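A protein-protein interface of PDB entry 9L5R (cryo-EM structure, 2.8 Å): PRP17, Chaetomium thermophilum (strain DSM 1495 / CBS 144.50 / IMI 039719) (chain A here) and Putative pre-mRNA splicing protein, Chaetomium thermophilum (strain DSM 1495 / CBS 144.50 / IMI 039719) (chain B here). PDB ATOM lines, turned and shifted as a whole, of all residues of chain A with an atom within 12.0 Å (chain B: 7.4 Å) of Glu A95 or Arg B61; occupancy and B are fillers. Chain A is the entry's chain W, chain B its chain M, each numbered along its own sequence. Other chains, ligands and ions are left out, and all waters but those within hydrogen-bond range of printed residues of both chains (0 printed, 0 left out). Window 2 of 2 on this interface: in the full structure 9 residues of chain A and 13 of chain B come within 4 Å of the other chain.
CE1 of Phe A87 touches CB of Tyr B32 (3.7 Å).
Lys A90 touches Tyr B32 (CD to OH, 3.2 Å).
Asn B30 touches His A91.
NE2 of His A91 touches CD of Lys B34, 3.4 Å away.
Val A94 touches Asn B30.
Asn B30 touches Glu A95.
Hydrophobic or aromatic side chains of chain A within 4 Å of the printed part of chain B: Phe A87, His A91 and Val A94.
Of the 13 printed residues of chain B, 4 touch a printed residue of chain A.
Hydrophobic or aromatic side chains of chain B within 4 Å of the printed part of chain A: Tyr B32.
Along chain B the printed residues that touch a printed residue of chain A span positions 30 to 61.
Glu A95 touches two residues of chain B.
Arg B61 touches one residue of chain A.
No residue of chain A comes within 4 Å of Ala B57.
No residue of chain A comes within 4 Å of Gly B58.
No residue of chain A comes within 4 Å of Gly B60.
No residue of chain A comes within 4 Å of Ala B62.
Printed residues of chain B within 4 Å of Phe A87: Tyr B32.
Of the printed residues of chain B, His A91 touches Asn B30, Tyr B32 and Lys B34.
Printed residues of chain A within 4 Å of Lys B34: His A91.
Of the printed residues of chain B, Lys A90 touches Tyr B32.
Printed residues of chain B within 4 Å of Val A94: Asn B30 (3.4 Å).
The nearest residue of chain B that does not touch Glu A95 is Lys B34 (4.7 Å).
The nearest residue of chain A that does not touch Arg B61 is His A91 (6.3 Å).
The nearest printed residue of chain B that does not touch Val A94 is Tyr B32 (4.02 Å).
The backbone carbonyl oxygen (O) of Tyr B32 sits close to a ring nitrogen (NE2) of His A91 (3.4 Å).
OE2 of Glu A95 lies within salt-bridge range of NH2 of Arg B61, 3.3 Å away.
The side-chain amide oxygen (OD1) of Asn B30 lies within hydrogen-bond range of the backbone NH (N) of Tyr B32 (3.0 Å).
A ring nitrogen (ND1) of His A91 is in hydrogen-bond range of the side-chain carboxylate (OE1) of Glu A95, 3.1 Å away.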
ATOM      1  N   GLU A  84      16.244   5.105  26.180  1.00  0.00           N
ATOM      2  CA  GLU A  84      17.356   5.569  26.997  1.00  0.00           C
ATOM      3  C   GLU A  84      18.584   5.848  26.147  1.00  0.00           C
ATOM      4  O   GLU A  84      19.306   6.821  26.386  1.00  0.00           O
ATOM      5  CB  GLU A  84      17.660   4.536  28.078  1.00  0.00           C
ATOM      6  CG  GLU A  84      18.682   4.991  29.091  1.00  0.00           C
ATOM      7  CD  GLU A  84      18.135   6.024  30.047  1.00  0.00           C
ATOM      8  OE1 GLU A  84      17.002   5.840  30.535  1.00  0.00           O
ATOM      9  OE2 GLU A  84      18.836   7.020  30.307  1.00  0.00           O
ATOM     10  N   ALA A  85      18.827   5.006  25.142  1.00  0.00           N
ATOM     11  CA  ALA A  85      19.938   5.227  24.226  1.00  0.00           C
ATOM     12  C   ALA A  85      19.744   6.499  23.419  1.00  0.00           C
ATOM     13  O   ALA A  85      20.708   7.226  23.161  1.00  0.00           O
ATOM     14  CB  ALA A  85      20.088   4.027  23.299  1.00  0.00           C
ATOM     15  N   THR A  86      18.503   6.775  23.008  1.00  0.00           N
ATOM     16  CA  THR A  86      18.190   8.012  22.301  1.00  0.00           C
ATOM     17  C   THR A  86      18.528   9.226  23.146  1.00  0.00           C
ATOM     18  O   THR A  86      19.212  10.150  22.682  1.00  0.00           O
ATOM     19  CB  THR A  86      16.710   8.043  21.920  1.00  0.00           C
ATOM     20  OG1 THR A  86      16.398   6.934  21.075  1.00  0.00           O
ATOM     21  CG2 THR A  86      16.376   9.324  21.198  1.00  0.00           C
ATOM     22  N   PHE A  87      18.069   9.227  24.405  1.00  0.00           N
ATOM     23  CA  PHE A  87      18.361  10.352  25.286  1.00  0.00           C
ATOM     24  C   PHE A  87      19.854  10.504  25.522  1.00  0.00           C
ATOM     25  O   PHE A  87      20.376  11.621  25.496  1.00  0.00           O
ATOM     26  CB  PHE A  87      17.640  10.211  26.626  1.00  0.00           C
ATOM     27  CG  PHE A  87      17.837  11.396  27.534  1.00  0.00           C
ATOM     28  CD1 PHE A  87      16.986  12.479  27.462  1.00  0.00           C
ATOM     29  CD2 PHE A  87      18.883  11.437  28.445  1.00  0.00           C
ATOM     30  CE1 PHE A  87      17.177  13.566  28.270  1.00  0.00           C
ATOM     31  CE2 PHE A  87      19.077  12.528  29.238  1.00  0.00           C
ATOM     32  CZ  PHE A  87      18.223  13.587  29.159  1.00  0.00           C
ATOM     33  N   ARG A  88      20.551   9.394  25.771  1.00  0.00           N
ATOM     34  CA  ARG A  88      21.972   9.476  26.081  1.00  0.00           C
ATOM     35  C   ARG A  88      22.772   9.964  24.884  1.00  0.00           C
ATOM     36  O   ARG A  88      23.698  10.763  25.039  1.00  0.00           O
ATOM     37  CB  ARG A  88      22.478   8.120  26.554  1.00  0.00           C
ATOM     38  CG  ARG A  88      22.274   7.871  28.030  1.00  0.00           C
ATOM     39  CD  ARG A  88      22.445   6.409  28.344  1.00  0.00           C
ATOM     40  NE  ARG A  88      22.072   6.082  29.711  1.00  0.00           N
ATOM     41  CZ  ARG A  88      22.932   5.968  30.711  1.00  0.00           C
ATOM     42  NH1 ARG A  88      24.227   6.168  30.533  1.00  0.00           N
ATOM     43  NH2 ARG A  88      22.481   5.649  31.920  1.00  0.00           N
ATOM     44  N   ALA A  89      22.395   9.535  23.680  1.00  0.00           N
ATOM     45  CA  ALA A  89      23.115   9.955  22.488  1.00  0.00           C
ATOM     46  C   ALA A  89      22.887  11.428  22.187  1.00  0.00           C
ATOM     47  O   ALA A  89      23.835  12.148  21.859  1.00  0.00           O
ATOM     48  CB  ALA A  89      22.702   9.094  21.301  1.00  0.00           C
ATOM     49  N   LYS A  90      21.640  11.898  22.286  1.00  0.00           N
ATOM     50  CA  LYS A  90      21.382  13.311  22.025  1.00  0.00           C
ATOM     51  C   LYS A  90      22.031  14.199  23.081  1.00  0.00           C
ATOM     52  O   LYS A  90      22.600  15.255  22.758  1.00  0.00           O
ATOM     53  CB  LYS A  90      19.881  13.551  21.952  1.00  0.00           C
ATOM     54  CG  LYS A  90      19.266  12.933  20.729  1.00  0.00           C
ATOM     55  CD  LYS A  90      17.796  13.228  20.615  1.00  0.00           C
ATOM     56  CE  LYS A  90      17.218  12.573  19.379  1.00  0.00           C
ATOM     57  NZ  LYS A  90      17.925  12.985  18.143  1.00  0.00           N
ATOM     58  N   HIS A  91      21.980  13.766  24.342  1.00  0.00           N
ATOM     59  CA  HIS A  91      22.638  14.493  25.415  1.00  0.00           C
ATOM     60  C   HIS A  91      24.139  14.560  25.194  1.00  0.00           C
ATOM     61  O   HIS A  91      24.754  15.602  25.420  1.00  0.00           O
ATOM     62  CB  HIS A  91      22.321  13.828  26.750  1.00  0.00           C
ATOM     63  CG  HIS A  91      22.650  14.670  27.936  1.00  0.00           C
ATOM     64  ND1 HIS A  91      23.941  14.901  28.354  1.00  0.00           N
ATOM     65  CD2 HIS A  91      21.851  15.336  28.797  1.00  0.00           C
ATOM     66  CE1 HIS A  91      23.921  15.677  29.420  1.00  0.00           C
ATOM     67  NE2 HIS A  91      22.666  15.956  29.709  1.00  0.00           N
ATOM     68  N   ARG A  92      24.739  13.461  24.739  1.00  0.00           N
ATOM     69  CA  ARG A  92      26.162  13.448  24.424  1.00  0.00           C
ATOM     70  C   ARG A  92      26.499  14.366  23.269  1.00  0.00           C
ATOM     71  O   ARG A  92      27.547  15.021  23.277  1.00  0.00           O
ATOM     72  CB  ARG A  92      26.598  12.031  24.106  1.00  0.00           C
ATOM     73  CG  ARG A  92      28.058  11.880  23.801  1.00  0.00           C
ATOM     74  CD  ARG A  92      28.829  12.226  25.014  1.00  0.00           C
ATOM     75  NE  ARG A  92      28.411  11.345  26.084  1.00  0.00           N
ATOM     76  CZ  ARG A  92      28.873  10.128  26.290  1.00  0.00           C
ATOM     77  NH1 ARG A  92      29.766   9.581  25.486  1.00  0.00           N
ATOM     78  NH2 ARG A  92      28.407   9.435  27.319  1.00  0.00           N
ATOM     79  N   ALA A  93      25.640  14.393  22.250  1.00  0.00           N
ATOM     80  CA  ALA A  93      25.888  15.241  21.094  1.00  0.00           C
ATOM     81  C   ALA A  93      25.915  16.702  21.496  1.00  0.00           C
ATOM     82  O   ALA A  93      26.741  17.475  21.000  1.00  0.00           O
ATOM     83  CB  ALA A  93      24.827  14.997  20.029  1.00  0.00           C
ATOM     84  N   VAL A  94      25.032  17.097  22.410  1.00  0.00           N
ATOM     85  CA  VAL A  94      25.081  18.474  22.893  1.00  0.00           C
ATOM     86  C   VAL A  94      26.252  18.679  23.857  1.00  0.00           C
ATOM     87  O   VAL A  94      26.939  19.703  23.805  1.00  0.00           O
ATOM     88  CB  VAL A  94      23.735  18.861  23.525  1.00  0.00           C
ATOM     89  CG1 VAL A  94      23.739  20.316  23.931  1.00  0.00           C
ATOM     90  CG2 VAL A  94      22.611  18.595  22.551  1.00  0.00           C
ATOM     91  N   GLU A  95      26.522  17.704  24.727  1.00  0.00           N
ATOM     92  CA  GLU A  95      27.373  17.901  25.896  1.00  0.00           C
ATOM     93  C   GLU A  95      28.862  17.729  25.640  1.00  0.00           C
ATOM     94  O   GLU A  95      29.666  18.416  26.277  1.00  0.00           O
ATOM     95  CB  GLU A  95      26.960  16.929  27.002  1.00  0.00           C
ATOM     96  CG  GLU A  95      27.435  17.321  28.384  1.00  0.00           C
ATOM     97  CD  GLU A  95      27.149  16.258  29.410  1.00  0.00           C
ATOM     98  OE1 GLU A  95      26.937  15.094  29.010  1.00  0.00           O
ATOM     99  OE2 GLU A  95      27.117  16.585  30.613  1.00  0.00           O
ATOM    100  N   ALA A  96      29.263  16.816  24.766  1.00  0.00           N
ATOM    101  CA  ALA A  96      30.682  16.656  24.493  1.00  0.00           C
ATOM    102  C   ALA A  96      31.194  17.838  23.688  1.00  0.00           C
ATOM    103  O   ALA A  96      30.458  18.452  22.912  1.00  0.00           O
ATOM    104  CB  ALA A  96      30.938  15.357  23.736  1.00  0.00           C
ATOM    105  N   VAL A  97      32.465  18.178  23.888  1.00  0.00           N
ATOM    106  CA  VAL A  97      33.069  19.200  23.048  1.00  0.00           C
ATOM    107  C   VAL A  97      33.405  18.592  21.692  1.00  0.00           C
ATOM    108  O   VAL A  97      33.551  17.377  21.542  1.00  0.00           O
ATOM    109  CB  VAL A  97      34.311  19.834  23.699  1.00  0.00           C
ATOM    110  CG1 VAL A  97      33.972  20.397  25.064  1.00  0.00           C
ATOM    111  CG2 VAL A  97      35.457  18.859  23.758  1.00  0.00           C
ATOM    112  N   GLY A  98      33.531  19.453  20.691  1.00  0.00           N
ATOM    113  CA  GLY A  98      33.717  18.973  19.335  1.00  0.00           C
ATOM    114  C   GLY A  98      32.509  18.260  18.768  1.00  0.00           C
ATOM    115  O   GLY A  98      32.655  17.182  18.178  1.00  0.00           O
ATOM    116  N   GLY A  99      31.319  18.825  18.956  1.00  0.00           N
ATOM    117  CA  GLY A  99      30.121  18.203  18.417  1.00  0.00           C
ATOM    118  C   GLY A  99      30.124  18.214  16.898  1.00  0.00           C
ATOM    119  O   GLY A  99      30.665  19.123  16.264  1.00  0.00           O
ATOM    120  N   GLY A 100      29.502  17.195  16.313  1.00  0.00           N
ATOM    121  CA  GLY A 100      29.619  17.001  14.877  1.00  0.00           C
ATOM    122  C   GLY A 100      31.040  16.598  14.542  1.00  0.00           C
ATOM    123  O   GLY A 100      31.548  15.587  15.041  1.00  0.00           O
ATOM    124  N   VAL A 101      31.689  17.415  13.707  1.00  0.00           N
ATOM    125  CA  VAL A 101      33.107  17.327  13.347  1.00  0.00           C
ATOM    126  C   VAL A 101      33.484  16.043  12.620  1.00  0.00           C
ATOM    127  O   VAL A 101      33.540  14.953  13.203  1.00  0.00           O
ATOM    128  CB  VAL A 101      34.025  17.539  14.563  1.00  0.00           C
ATOM    129  CG1 VAL A 101      35.468  17.545  14.104  1.00  0.00           C
ATOM    130  CG2 VAL A 101      33.719  18.870  15.211  1.00  0.00           C
ATOM    131  N   GLU B  29      21.377  24.964  29.483  1.00  0.00           N
ATOM    132  CA  GLU B  29      21.432  25.287  28.060  1.00  0.00           C
ATOM    133  C   GLU B  29      21.244  24.049  27.195  1.00  0.00           C
ATOM    134  O   GLU B  29      20.700  24.145  26.091  1.00  0.00           O
ATOM    135  CB  GLU B  29      22.749  25.984  27.719  1.00  0.00           C
ATOM    136  CG  GLU B  29      23.994  25.242  28.153  1.00  0.00           C
ATOM    137  CD  GLU B  29      24.581  24.377  27.052  1.00  0.00           C
ATOM    138  OE1 GLU B  29      24.164  24.529  25.885  1.00  0.00           O
ATOM    139  OE2 GLU B  29      25.464  23.547  27.352  1.00  0.00           O
ATOM    140  N   ASN B  30      21.700  22.897  27.671  1.00  0.00           N
ATOM    141  CA  ASN B  30      21.455  21.621  27.023  1.00  0.00           C
ATOM    142  C   ASN B  30      19.957  21.364  26.987  1.00  0.00           C
ATOM    143  O   ASN B  30      19.317  21.365  28.046  1.00  0.00           O
ATOM    144  CB  ASN B  30      22.170  20.518  27.800  1.00  0.00           C
ATOM    145  CG  ASN B  30      22.366  19.247  27.001  1.00  0.00           C
ATOM    146  OD1 ASN B  30      21.434  18.704  26.419  1.00  0.00           O
ATOM    147  ND2 ASN B  30      23.593  18.758  26.989  1.00  0.00           N
ATOM    148  N   TYR B  32      18.424  18.715  26.757  1.00  0.00           N
ATOM    149  CA  TYR B  32      18.149  17.401  27.318  1.00  0.00           C
ATOM    150  C   TYR B  32      18.559  17.454  28.780  1.00  0.00           C
ATOM    151  O   TYR B  32      19.746  17.575  29.092  1.00  0.00           O
ATOM    152  CB  TYR B  32      18.912  16.332  26.545  1.00  0.00           C
ATOM    153  CG  TYR B  32      18.524  16.326  25.097  1.00  0.00           C
ATOM    154  CD1 TYR B  32      17.368  15.695  24.674  1.00  0.00           C
ATOM    155  CD2 TYR B  32      19.291  16.989  24.155  1.00  0.00           C
ATOM    156  CE1 TYR B  32      17.000  15.707  23.355  1.00  0.00           C
ATOM    157  CE2 TYR B  32      18.928  17.013  22.837  1.00  0.00           C
ATOM    158  CZ  TYR B  32      17.781  16.367  22.441  1.00  0.00           C
ATOM    159  OH  TYR B  32      17.409  16.383  21.121  1.00  0.00           O
ATOM    160  N   LYS B  34      18.726  16.334  32.798  1.00  0.00           N
ATOM    161  CA  LYS B  34      18.795  15.293  33.811  1.00  0.00           C
ATOM    162  C   LYS B  34      18.368  15.904  35.147  1.00  0.00           C
ATOM    163  O   LYS B  34      19.157  16.584  35.804  1.00  0.00           O
ATOM    164  CB  LYS B  34      20.214  14.739  33.873  1.00  0.00           C
ATOM    165  CG  LYS B  34      20.581  13.796  32.758  1.00  0.00           C
ATOM    166  CD  LYS B  34      22.020  13.987  32.353  1.00  0.00           C
ATOM    167  CE  LYS B  34      22.955  13.164  33.195  1.00  0.00           C
ATOM    168  NZ  LYS B  34      24.364  13.584  33.045  1.00  0.00           N
ATOM    169  N   ALA B  57      21.863  19.398  37.500  1.00  0.00           N
ATOM    170  CA  ALA B  57      23.248  19.820  37.384  1.00  0.00           C
ATOM    171  C   ALA B  57      23.358  20.886  36.312  1.00  0.00           C
ATOM    172  O   ALA B  57      22.739  20.784  35.250  1.00  0.00           O
ATOM    173  CB  ALA B  57      24.153  18.638  37.047  1.00  0.00           C
ATOM    174  N   GLY B  58      24.152  21.908  36.598  1.00  0.00           N
ATOM    175  CA  GLY B  58      24.181  23.092  35.771  1.00  0.00           C
ATOM    176  C   GLY B  58      24.900  22.889  34.452  1.00  0.00           C
ATOM    177  O   GLY B  58      24.929  21.813  33.856  1.00  0.00           O
ATOM    178  N   ASP B  59      25.491  23.982  33.978  1.00  0.00           N
ATOM    179  CA  ASP B  59      26.092  23.970  32.654  1.00  0.00           C
ATOM    180  C   ASP B  59      27.607  23.825  32.701  1.00  0.00           C
ATOM    181  O   ASP B  59      28.192  23.237  31.786  1.00  0.00           O
ATOM    182  CB  ASP B  59      25.701  25.244  31.911  1.00  0.00           C
ATOM    183  CG  ASP B  59      24.216  25.324  31.654  1.00  0.00           C
ATOM    184  OD1 ASP B  59      23.610  24.270  31.387  1.00  0.00           O
ATOM    185  OD2 ASP B  59      23.654  26.436  31.719  1.00  0.00           O
ATOM    186  N   GLY B  60      28.255  24.339  33.746  1.00  0.00           N
ATOM    187  CA  GLY B  60      29.698  24.457  33.763  1.00  0.00           C
ATOM    188  C   GLY B  60      30.454  23.604  34.752  1.00  0.00           C
ATOM    189  O   GLY B  60      31.654  23.842  34.947  1.00  0.00           O
ATOM    190  N   ARG B  61      29.810  22.610  35.374  1.00  0.00           N
ATOM    191  CA  ARG B  61      30.410  21.752  36.407  1.00  0.00           C
ATOM    192  C   ARG B  61      30.993  22.579  37.546  1.00  0.00           C
ATOM    193  O   ARG B  61      32.052  22.266  38.092  1.00  0.00           O
ATOM    194  CB  ARG B  61      31.463  20.807  35.821  1.00  0.00           C
ATOM    195  CG  ARG B  61      30.938  19.897  34.730  1.00  0.00           C
ATOM    196  CD  ARG B  61      30.772  18.472  35.204  1.00  0.00           C
ATOM    197  NE  ARG B  61      30.219  17.628  34.155  1.00  0.00           N
ATOM    198  CZ  ARG B  61      29.302  16.693  34.345  1.00  0.00           C
ATOM    199  NH1 ARG B  61      28.807  16.443  35.540  1.00  0.00           N
ATOM    200  NH2 ARG B  61      28.868  15.994  33.306  1.00  0.00           N
ATOM    201  N   ALA B  62      30.300  23.663  37.889  1.00  0.00           N
ATOM    202  CA  ALA B  62      30.669  24.472  39.037  1.00  0.00           C
ATOM    203  C   ALA B  62      30.491  23.656  40.306  1.00  0.00           C
ATOM    204  O   ALA B  62      29.663  22.741  40.362  1.00  0.00           O
ATOM    205  CB  ALA B  62      29.816  25.737  39.099  1.00  0.00           C
ATOM    206  N   HIS B  63      31.306  23.968  41.315  1.00  0.00           N
ATOM    207  CA  HIS B  63      31.315  23.169  42.533  1.00  0.00           C
ATOM    208  C   HIS B  63      29.958  23.198  43.211  1.00  0.00           C
ATOM    209  O   HIS B  63      29.268  22.173  43.208  1.00  0.00           O
ATOM    210  CB  HIS B  63      32.391  23.659  43.496  1.00  0.00           C
ATOM    211  CG  HIS B  63      32.348  22.985  44.829  1.00  0.00           C
ATOM    212  ND1 HIS B  63      32.347  21.613  44.969  1.00  0.00           N
ATOM    213  CD2 HIS B  63      32.306  23.492  46.084  1.00  0.00           C
ATOM    214  CE1 HIS B  63      32.303  21.306  46.254  1.00  0.00           C
ATOM    215  NE2 HIS B  63      32.280  22.427  46.951  1.00  0.00           N
ATOM    216  N   GLY B  64      29.581  24.364  43.754  1.00  0.00           N
ATOM    217  CA  GLY B  64      28.231  24.750  44.150  1.00  0.00           C
ATOM    218  C   GLY B  64      27.322  23.661  44.671  1.00  0.00           C
ATOM    219  O   GLY B  64      27.694  22.903  45.571  1.00  0.00           O
ATOM    220  N   LYS B  66      23.499  21.520  42.747  1.00  0.00           N
ATOM    221  CA  LYS B  66      22.567  21.531  41.643  1.00  0.00           C
ATOM    222  C   LYS B  66      21.578  22.672  41.830  1.00  0.00           C
ATOM    223  O   LYS B  66      21.243  23.051  42.953  1.00  0.00           O
ATOM    224  CB  LYS B  66      21.848  20.190  41.566  1.00  0.00           C
ATOM    225  CG  LYS B  66      22.806  19.063  41.300  1.00  0.00           C
ATOM    226  CD  LYS B  66      22.117  17.733  41.150  1.00  0.00           C
ATOM    227  CE  LYS B  66      22.918  16.831  40.213  1.00  0.00           C
ATOM    228  NZ  LYS B  66      24.090  16.203  40.887  1.00  0.00           N
